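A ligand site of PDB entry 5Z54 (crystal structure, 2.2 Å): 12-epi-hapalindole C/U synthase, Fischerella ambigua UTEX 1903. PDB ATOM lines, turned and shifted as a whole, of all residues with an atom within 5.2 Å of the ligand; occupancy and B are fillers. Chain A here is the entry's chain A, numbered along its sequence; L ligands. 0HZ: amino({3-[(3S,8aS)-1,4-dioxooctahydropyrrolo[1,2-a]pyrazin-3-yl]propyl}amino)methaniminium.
The side-chain amide oxygen (OD1) of Asn 76 sits close to the side-chain hydroxyl (OH) of Tyr 101 (3.2 Å). N of Tyr 103 lies within hydrogen-bond range of O of Asn 76 (2.8 Å). ND2 of Asn 76 is in hydrogen-bond range of O of Thr 74, at 3.3 Å. The side-chain amide nitrogen of Asn 76 lies within hydrogen-bond range of the backbone carbonyl oxygen of Thr 71 (3.2 Å). The side-chain hydroxyl of Tyr 89 lies within hydrogen-bond range of the backbone NH of Phe 138 (3.3 Å).
Residues that only touch the ligand: Tyr 49 (3.5 Å), Thr 72 (3.6 Å), Phe 88 (3.4 Å), Tyr 101 (3.6 Å), Tyr 103 (3.8 Å), Phe 138 (3.3 Å) and Phe 210 (3.5 Å). Hydrophobic or aromatic side chains that line the ligand: Tyr 49, Phe 88, Tyr 101, Tyr 103, Phe 138 and Phe 210. Within 4 Å of the ligand: Tyr 49, Thr 72, Asn 76, Phe 88, Tyr 101, Tyr 103, Phe 138, Phe 210 and Asp 214. The nearest printed residue that does not touch the ligand is Ile 99 (4.02 Å).
O of the ligand lies within hydrogen-bond range of ND2 of Asn 76. The side-chain carboxylate (OD1) of Asp 214 lies within salt-bridge range of a nitrogen (NH2) of the ligand (3.1 Å).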
ATOM      1  N   ASP A  47     -23.318  -2.100 -27.163  1.00  0.00           N
ATOM      2  CA  ASP A  47     -22.906  -3.263 -26.355  1.00  0.00           C
ATOM      3  C   ASP A  47     -21.567  -3.039 -25.689  1.00  0.00           C
ATOM      4  O   ASP A  47     -20.997  -3.972 -25.160  1.00  0.00           O
ATOM      5  CB  ASP A  47     -22.865  -4.574 -27.129  1.00  0.00           C
ATOM      6  CG  ASP A  47     -24.257  -5.028 -27.565  1.00  0.00           C
ATOM      7  OD1 ASP A  47     -25.249  -4.599 -26.899  1.00  0.00           O
ATOM      8  OD2 ASP A  47     -24.358  -5.812 -28.560  1.00  0.00           O
ATOM      9  N   TYR A  49     -19.239  -1.379 -22.582  1.00  0.00           N
ATOM     10  CA  TYR A  49     -19.482  -1.431 -21.138  1.00  0.00           C
ATOM     11  C   TYR A  49     -18.240  -0.962 -20.400  1.00  0.00           C
ATOM     12  O   TYR A  49     -17.161  -0.997 -20.965  1.00  0.00           O
ATOM     13  CB  TYR A  49     -19.884  -2.844 -20.724  1.00  0.00           C
ATOM     14  CG  TYR A  49     -18.879  -3.892 -21.134  1.00  0.00           C
ATOM     15  CD1 TYR A  49     -18.921  -4.481 -22.388  1.00  0.00           C
ATOM     16  CD2 TYR A  49     -17.855  -4.257 -20.260  1.00  0.00           C
ATOM     17  CE1 TYR A  49     -17.995  -5.435 -22.756  1.00  0.00           C
ATOM     18  CE2 TYR A  49     -16.917  -5.219 -20.618  1.00  0.00           C
ATOM     19  CZ  TYR A  49     -17.002  -5.812 -21.869  1.00  0.00           C
ATOM     20  OH  TYR A  49     -16.091  -6.750 -22.235  1.00  0.00           O
ATOM     21  N   VAL A  51     -15.988  -1.594 -16.691  1.00  0.00           N
ATOM     22  CA  VAL A  51     -15.703  -2.705 -15.806  1.00  0.00           C
ATOM     23  C   VAL A  51     -15.415  -2.132 -14.429  1.00  0.00           C
ATOM     24  O   VAL A  51     -14.792  -2.790 -13.614  1.00  0.00           O
ATOM     25  CB  VAL A  51     -14.532  -3.563 -16.316  1.00  0.00           C
ATOM     26  CG1 VAL A  51     -14.862  -4.306 -17.602  1.00  0.00           C
ATOM     27  CG2 VAL A  51     -13.225  -2.789 -16.451  1.00  0.00           C
ATOM     28  N   THR A  71     -10.565  -6.596 -15.002  1.00  0.00           N
ATOM     29  CA  THR A  71     -10.313  -6.801 -16.430  1.00  0.00           C
ATOM     30  C   THR A  71     -11.393  -7.712 -17.019  1.00  0.00           C
ATOM     31  O   THR A  71     -12.198  -8.291 -16.286  1.00  0.00           O
ATOM     32  CB  THR A  71      -8.919  -7.437 -16.632  1.00  0.00           C
ATOM     33  OG1 THR A  71      -8.937  -8.859 -16.478  1.00  0.00           O
ATOM     34  CG2 THR A  71      -7.882  -6.868 -15.703  1.00  0.00           C
ATOM     35  N   THR A  72     -11.377  -7.862 -18.353  1.00  0.00           N
ATOM     36  CA  THR A  72     -12.101  -8.847 -19.127  1.00  0.00           C
ATOM     37  C   THR A  72     -12.017 -10.245 -18.509  1.00  0.00           C
ATOM     38  O   THR A  72     -12.950 -11.030 -18.584  1.00  0.00           O
ATOM     39  CB  THR A  72     -11.489  -8.916 -20.537  1.00  0.00           C
ATOM     40  OG1 THR A  72     -11.454  -7.577 -21.028  1.00  0.00           O
ATOM     41  CG2 THR A  72     -12.196  -9.846 -21.524  1.00  0.00           C
ATOM     42  N   THR A  74     -11.695 -11.279 -15.493  1.00  0.00           N
ATOM     43  CA  THR A  74     -12.069 -11.429 -14.099  1.00  0.00           C
ATOM     44  C   THR A  74     -13.559 -11.141 -13.915  1.00  0.00           C
ATOM     45  O   THR A  74     -14.214 -10.607 -14.814  1.00  0.00           O
ATOM     46  CB  THR A  74     -11.264 -10.496 -13.181  1.00  0.00           C
ATOM     47  OG1 THR A  74     -11.647  -9.106 -13.355  1.00  0.00           O
ATOM     48  CG2 THR A  74      -9.767 -10.665 -13.306  1.00  0.00           C
ATOM     49  N   ASN A  76     -16.437  -8.823 -12.533  1.00  0.00           N
ATOM     50  CA  ASN A  76     -16.492  -7.385 -12.611  1.00  0.00           C
ATOM     51  C   ASN A  76     -17.949  -6.949 -12.597  1.00  0.00           C
ATOM     52  O   ASN A  76     -18.873  -7.776 -12.711  1.00  0.00           O
ATOM     53  CB  ASN A  76     -15.767  -6.838 -13.848  1.00  0.00           C
ATOM     54  CG  ASN A  76     -16.252  -7.481 -15.143  1.00  0.00           C
ATOM     55  OD1 ASN A  76     -17.438  -7.688 -15.330  1.00  0.00           O
ATOM     56  ND2 ASN A  76     -15.341  -7.799 -16.042  1.00  0.00           N
ATOM     57  N   GLY A  80     -23.420  -0.810 -19.030  1.00  0.00           N
ATOM     58  CA  GLY A  80     -23.402  -1.258 -20.421  1.00  0.00           C
ATOM     59  C   GLY A  80     -24.509  -0.562 -21.210  1.00  0.00           C
ATOM     60  O   GLY A  80     -25.585  -0.310 -20.658  1.00  0.00           O
ATOM     61  N   TYR A  81     -24.218  -0.188 -22.462  1.00  0.00           N
ATOM     62  CA  TYR A  81     -25.194   0.419 -23.347  1.00  0.00           C
ATOM     63  C   TYR A  81     -25.987  -0.666 -24.049  1.00  0.00           C
ATOM     64  O   TYR A  81     -25.420  -1.623 -24.580  1.00  0.00           O
ATOM     65  CB  TYR A  81     -24.477   1.400 -24.280  1.00  0.00           C
ATOM     66  CG  TYR A  81     -25.298   1.974 -25.410  1.00  0.00           C
ATOM     67  CD1 TYR A  81     -26.597   2.428 -25.205  1.00  0.00           C
ATOM     68  CD2 TYR A  81     -24.739   2.098 -26.682  1.00  0.00           C
ATOM     69  CE1 TYR A  81     -27.342   2.938 -26.256  1.00  0.00           C
ATOM     70  CE2 TYR A  81     -25.472   2.615 -27.750  1.00  0.00           C
ATOM     71  CZ  TYR A  81     -26.775   3.032 -27.523  1.00  0.00           C
ATOM     72  OH  TYR A  81     -27.490   3.508 -28.567  1.00  0.00           O
ATOM     73  N   VAL A  82     -27.333  -0.531 -23.994  1.00  0.00           N
ATOM     74  CA  VAL A  82     -28.256  -1.439 -24.674  1.00  0.00           C
ATOM     75  C   VAL A  82     -29.095  -0.619 -25.658  1.00  0.00           C
ATOM     76  O   VAL A  82     -30.113  -0.051 -25.276  1.00  0.00           O
ATOM     77  CB  VAL A  82     -29.189  -2.219 -23.704  1.00  0.00           C
ATOM     78  CG1 VAL A  82     -30.048  -3.205 -24.486  1.00  0.00           C
ATOM     79  CG2 VAL A  82     -28.440  -2.962 -22.601  1.00  0.00           C
ATOM     80  N   PHE A  88     -27.603  -8.747 -27.146  1.00  0.00           N
ATOM     81  CA  PHE A  88     -27.851  -9.294 -25.804  1.00  0.00           C
ATOM     82  C   PHE A  88     -29.322  -9.327 -25.462  1.00  0.00           C
ATOM     83  O   PHE A  88     -29.731 -10.042 -24.551  1.00  0.00           O
ATOM     84  CB  PHE A  88     -27.248  -8.405 -24.716  1.00  0.00           C
ATOM     85  CG  PHE A  88     -25.743  -8.342 -24.746  1.00  0.00           C
ATOM     86  CD1 PHE A  88     -24.993  -9.489 -24.954  1.00  0.00           C
ATOM     87  CD2 PHE A  88     -25.082  -7.131 -24.571  1.00  0.00           C
ATOM     88  CE1 PHE A  88     -23.605  -9.435 -24.971  1.00  0.00           C
ATOM     89  CE2 PHE A  88     -23.692  -7.074 -24.598  1.00  0.00           C
ATOM     90  CZ  PHE A  88     -22.959  -8.236 -24.811  1.00  0.00           C
ATOM     91  N   TYR A  89     -30.106  -8.502 -26.138  1.00  0.00           N
ATOM     92  CA  TYR A  89     -31.462  -8.330 -25.714  1.00  0.00           C
ATOM     93  C   TYR A  89     -32.366  -8.368 -26.920  1.00  0.00           C
ATOM     94  O   TYR A  89     -31.921  -8.076 -28.025  1.00  0.00           O
ATOM     95  CB  TYR A  89     -31.570  -7.054 -24.874  1.00  0.00           C
ATOM     96  CG  TYR A  89     -31.093  -7.256 -23.469  1.00  0.00           C
ATOM     97  CD1 TYR A  89     -31.797  -8.092 -22.605  1.00  0.00           C
ATOM     98  CD2 TYR A  89     -29.928  -6.687 -23.019  1.00  0.00           C
ATOM     99  CE1 TYR A  89     -31.374  -8.325 -21.308  1.00  0.00           C
ATOM    100  CE2 TYR A  89     -29.473  -6.919 -21.727  1.00  0.00           C
ATOM    101  CZ  TYR A  89     -30.202  -7.728 -20.880  1.00  0.00           C
ATOM    102  OH  TYR A  89     -29.783  -7.969 -19.606  1.00  0.00           O
ATOM    103  N   ILE A  99     -27.687  -0.066 -18.738  1.00  0.00           N
ATOM    104  CA  ILE A  99     -28.072  -0.941 -17.663  1.00  0.00           C
ATOM    105  C   ILE A  99     -26.842  -1.069 -16.781  1.00  0.00           C
ATOM    106  O   ILE A  99     -25.773  -0.741 -17.245  1.00  0.00           O
ATOM    107  CB  ILE A  99     -28.619  -2.298 -18.186  1.00  0.00           C
ATOM    108  CG1 ILE A  99     -27.597  -3.116 -19.017  1.00  0.00           C
ATOM    109  CG2 ILE A  99     -29.919  -2.087 -18.946  1.00  0.00           C
ATOM    110  CD1 ILE A  99     -26.335  -3.503 -18.293  1.00  0.00           C
ATOM    111  N   TYR A 101     -24.525  -3.942 -14.621  1.00  0.00           N
ATOM    112  CA  TYR A 101     -24.403  -5.395 -14.693  1.00  0.00           C
ATOM    113  C   TYR A 101     -23.391  -5.915 -13.690  1.00  0.00           C
ATOM    114  O   TYR A 101     -22.501  -5.185 -13.272  1.00  0.00           O
ATOM    115  CB  TYR A 101     -23.979  -5.848 -16.091  1.00  0.00           C
ATOM    116  CG  TYR A 101     -22.502  -5.632 -16.308  1.00  0.00           C
ATOM    117  CD1 TYR A 101     -22.017  -4.410 -16.754  1.00  0.00           C
ATOM    118  CD2 TYR A 101     -21.585  -6.611 -15.959  1.00  0.00           C
ATOM    119  CE1 TYR A 101     -20.657  -4.185 -16.881  1.00  0.00           C
ATOM    120  CE2 TYR A 101     -20.219  -6.390 -16.055  1.00  0.00           C
ATOM    121  CZ  TYR A 101     -19.751  -5.186 -16.549  1.00  0.00           C
ATOM    122  OH  TYR A 101     -18.391  -4.978 -16.701  1.00  0.00           O
ATOM    123  N   TYR A 103     -21.001  -9.451 -13.354  1.00  0.00           N
ATOM    124  CA  TYR A 103     -20.567 -10.677 -13.994  1.00  0.00           C
ATOM    125  C   TYR A 103     -19.620 -11.413 -13.039  1.00  0.00           C
ATOM    126  O   TYR A 103     -18.630 -10.841 -12.570  1.00  0.00           O
ATOM    127  CB  TYR A 103     -19.872 -10.389 -15.335  1.00  0.00           C
ATOM    128  CG  TYR A 103     -19.132 -11.607 -15.818  1.00  0.00           C
ATOM    129  CD1 TYR A 103     -19.828 -12.780 -16.031  1.00  0.00           C
ATOM    130  CD2 TYR A 103     -17.758 -11.615 -15.934  1.00  0.00           C
ATOM    131  CE1 TYR A 103     -19.171 -13.955 -16.371  1.00  0.00           C
ATOM    132  CE2 TYR A 103     -17.077 -12.776 -16.309  1.00  0.00           C
ATOM    133  CZ  TYR A 103     -17.798 -13.936 -16.522  1.00  0.00           C
ATOM    134  OH  TYR A 103     -17.178 -15.089 -16.873  1.00  0.00           O
ATOM    135  N   PHE A 138     -29.263 -11.231 -19.813  1.00  0.00           N
ATOM    136  CA  PHE A 138     -28.759 -11.078 -21.168  1.00  0.00           C
ATOM    137  C   PHE A 138     -28.475 -12.454 -21.790  1.00  0.00           C
ATOM    138  O   PHE A 138     -28.061 -13.389 -21.117  1.00  0.00           O
ATOM    139  CB  PHE A 138     -27.660 -10.030 -21.301  1.00  0.00           C
ATOM    140  CG  PHE A 138     -26.409 -10.256 -20.490  1.00  0.00           C
ATOM    141  CD1 PHE A 138     -26.318  -9.754 -19.197  1.00  0.00           C
ATOM    142  CD2 PHE A 138     -25.321 -10.908 -21.047  1.00  0.00           C
ATOM    143  CE1 PHE A 138     -25.151  -9.930 -18.458  1.00  0.00           C
ATOM    144  CE2 PHE A 138     -24.172 -11.102 -20.305  1.00  0.00           C
ATOM    145  CZ  PHE A 138     -24.085 -10.623 -19.007  1.00  0.00           C
ATOM    146  N   ILE A 145     -18.651 -18.531 -26.435  1.00  0.00           N
ATOM    147  CA  ILE A 145     -19.133 -18.385 -25.041  1.00  0.00           C
ATOM    148  C   ILE A 145     -20.643 -18.128 -25.136  1.00  0.00           C
ATOM    149  O   ILE A 145     -21.033 -17.160 -25.768  1.00  0.00           O
ATOM    150  CB  ILE A 145     -18.404 -17.225 -24.341  1.00  0.00           C
ATOM    151  CG1 ILE A 145     -16.889 -17.459 -24.302  1.00  0.00           C
ATOM    152  CG2 ILE A 145     -18.968 -17.021 -22.945  1.00  0.00           C
ATOM    153  CD1 ILE A 145     -16.146 -16.522 -23.402  1.00  0.00           C
ATOM    154  N   LEU A 147     -24.306 -17.034 -23.608  1.00  0.00           N
ATOM    155  CA  LEU A 147     -24.787 -16.213 -22.466  1.00  0.00           C
ATOM    156  C   LEU A 147     -26.118 -16.780 -21.987  1.00  0.00           C
ATOM    157  O   LEU A 147     -26.721 -16.212 -21.083  1.00  0.00           O
ATOM    158  CB  LEU A 147     -24.850 -14.756 -22.902  1.00  0.00           C
ATOM    159  CG  LEU A 147     -23.534 -14.234 -23.454  1.00  0.00           C
ATOM    160  CD1 LEU A 147     -23.594 -12.752 -23.729  1.00  0.00           C
ATOM    161  CD2 LEU A 147     -22.398 -14.553 -22.514  1.00  0.00           C
ATOM    162  N   PHE A 210     -25.060 -19.046 -17.722  1.00  0.00           N
ATOM    163  CA  PHE A 210     -24.027 -18.013 -17.660  1.00  0.00           C
ATOM    164  C   PHE A 210     -24.279 -17.059 -16.477  1.00  0.00           C
ATOM    165  O   PHE A 210     -25.401 -16.647 -16.247  1.00  0.00           O
ATOM    166  CB  PHE A 210     -24.043 -17.267 -18.983  1.00  0.00           C
ATOM    167  CG  PHE A 210     -23.005 -16.183 -19.075  1.00  0.00           C
ATOM    168  CD1 PHE A 210     -21.683 -16.489 -19.347  1.00  0.00           C
ATOM    169  CD2 PHE A 210     -23.342 -14.845 -18.820  1.00  0.00           C
ATOM    170  CE1 PHE A 210     -20.719 -15.499 -19.408  1.00  0.00           C
ATOM    171  CE2 PHE A 210     -22.378 -13.854 -18.881  1.00  0.00           C
ATOM    172  CZ  PHE A 210     -21.070 -14.173 -19.169  1.00  0.00           C
ATOM    173  N   ASP A 214     -28.294  -8.087 -15.276  1.00  0.00           N
ATOM    174  CA  ASP A 214     -28.346  -6.644 -15.434  1.00  0.00           C
ATOM    175  C   ASP A 214     -29.484  -6.107 -14.568  1.00  0.00           C
ATOM    176  O   ASP A 214     -30.416  -6.831 -14.206  1.00  0.00           O
ATOM    177  CB  ASP A 214     -28.555  -6.254 -16.915  1.00  0.00           C
ATOM    178  CG  ASP A 214     -27.450  -6.753 -17.881  1.00  0.00           C
ATOM    179  OD1 ASP A 214     -26.292  -6.848 -17.435  1.00  0.00           O
ATOM    180  OD2 ASP A 214     -27.751  -7.014 -19.117  1.00  0.00           O
HETATM  181  N   0HZ L   1     -18.688 -10.562 -19.865  1.00  0.00           N
HETATM  182  CA  0HZ L   1     -17.365  -9.941 -20.064  1.00  0.00           C
HETATM  183  CB  0HZ L   1     -16.425 -11.152 -20.281  1.00  0.00           C
HETATM  184  CG  0HZ L   1     -17.270 -12.169 -20.985  1.00  0.00           C
HETATM  185  CD  0HZ L   1     -18.684 -11.951 -20.445  1.00  0.00           C
HETATM  186  C   0HZ L   1     -17.078  -9.149 -18.896  1.00  0.00           C
HETATM  187  O   0HZ L   1     -15.916  -8.980 -18.484  1.00  0.00           O
HETATM  188  N1  0HZ L   1     -18.207  -8.479 -18.216  1.00  0.00           N
HETATM  189  CA1 0HZ L   1     -19.604  -8.641 -18.741  1.00  0.00           C
HETATM  190  C1  0HZ L   1     -19.719  -9.937 -19.286  1.00  0.00           C
HETATM  191  O1  0HZ L   1     -20.757 -10.566 -19.174  1.00  0.00           O
HETATM  192  CB1 0HZ L   1     -19.856  -7.576 -19.777  1.00  0.00           C
HETATM  193  CG1 0HZ L   1     -21.323  -7.490 -20.153  1.00  0.00           C
HETATM  194  CD1 0HZ L   1     -21.588  -6.001 -20.423  1.00  0.00           C
HETATM  195  NE  0HZ L   1     -22.878  -5.680 -21.125  1.00  0.00           N
HETATM  196  CZ  0HZ L   1     -24.102  -6.078 -20.791  1.00  0.00           C
HETATM  197  NH1 0HZ L   1     -25.125  -5.615 -21.497  1.00  0.00           N
HETATM  198  NH2 0HZ L   1     -24.305  -6.977 -19.790  1.00  0.00           N
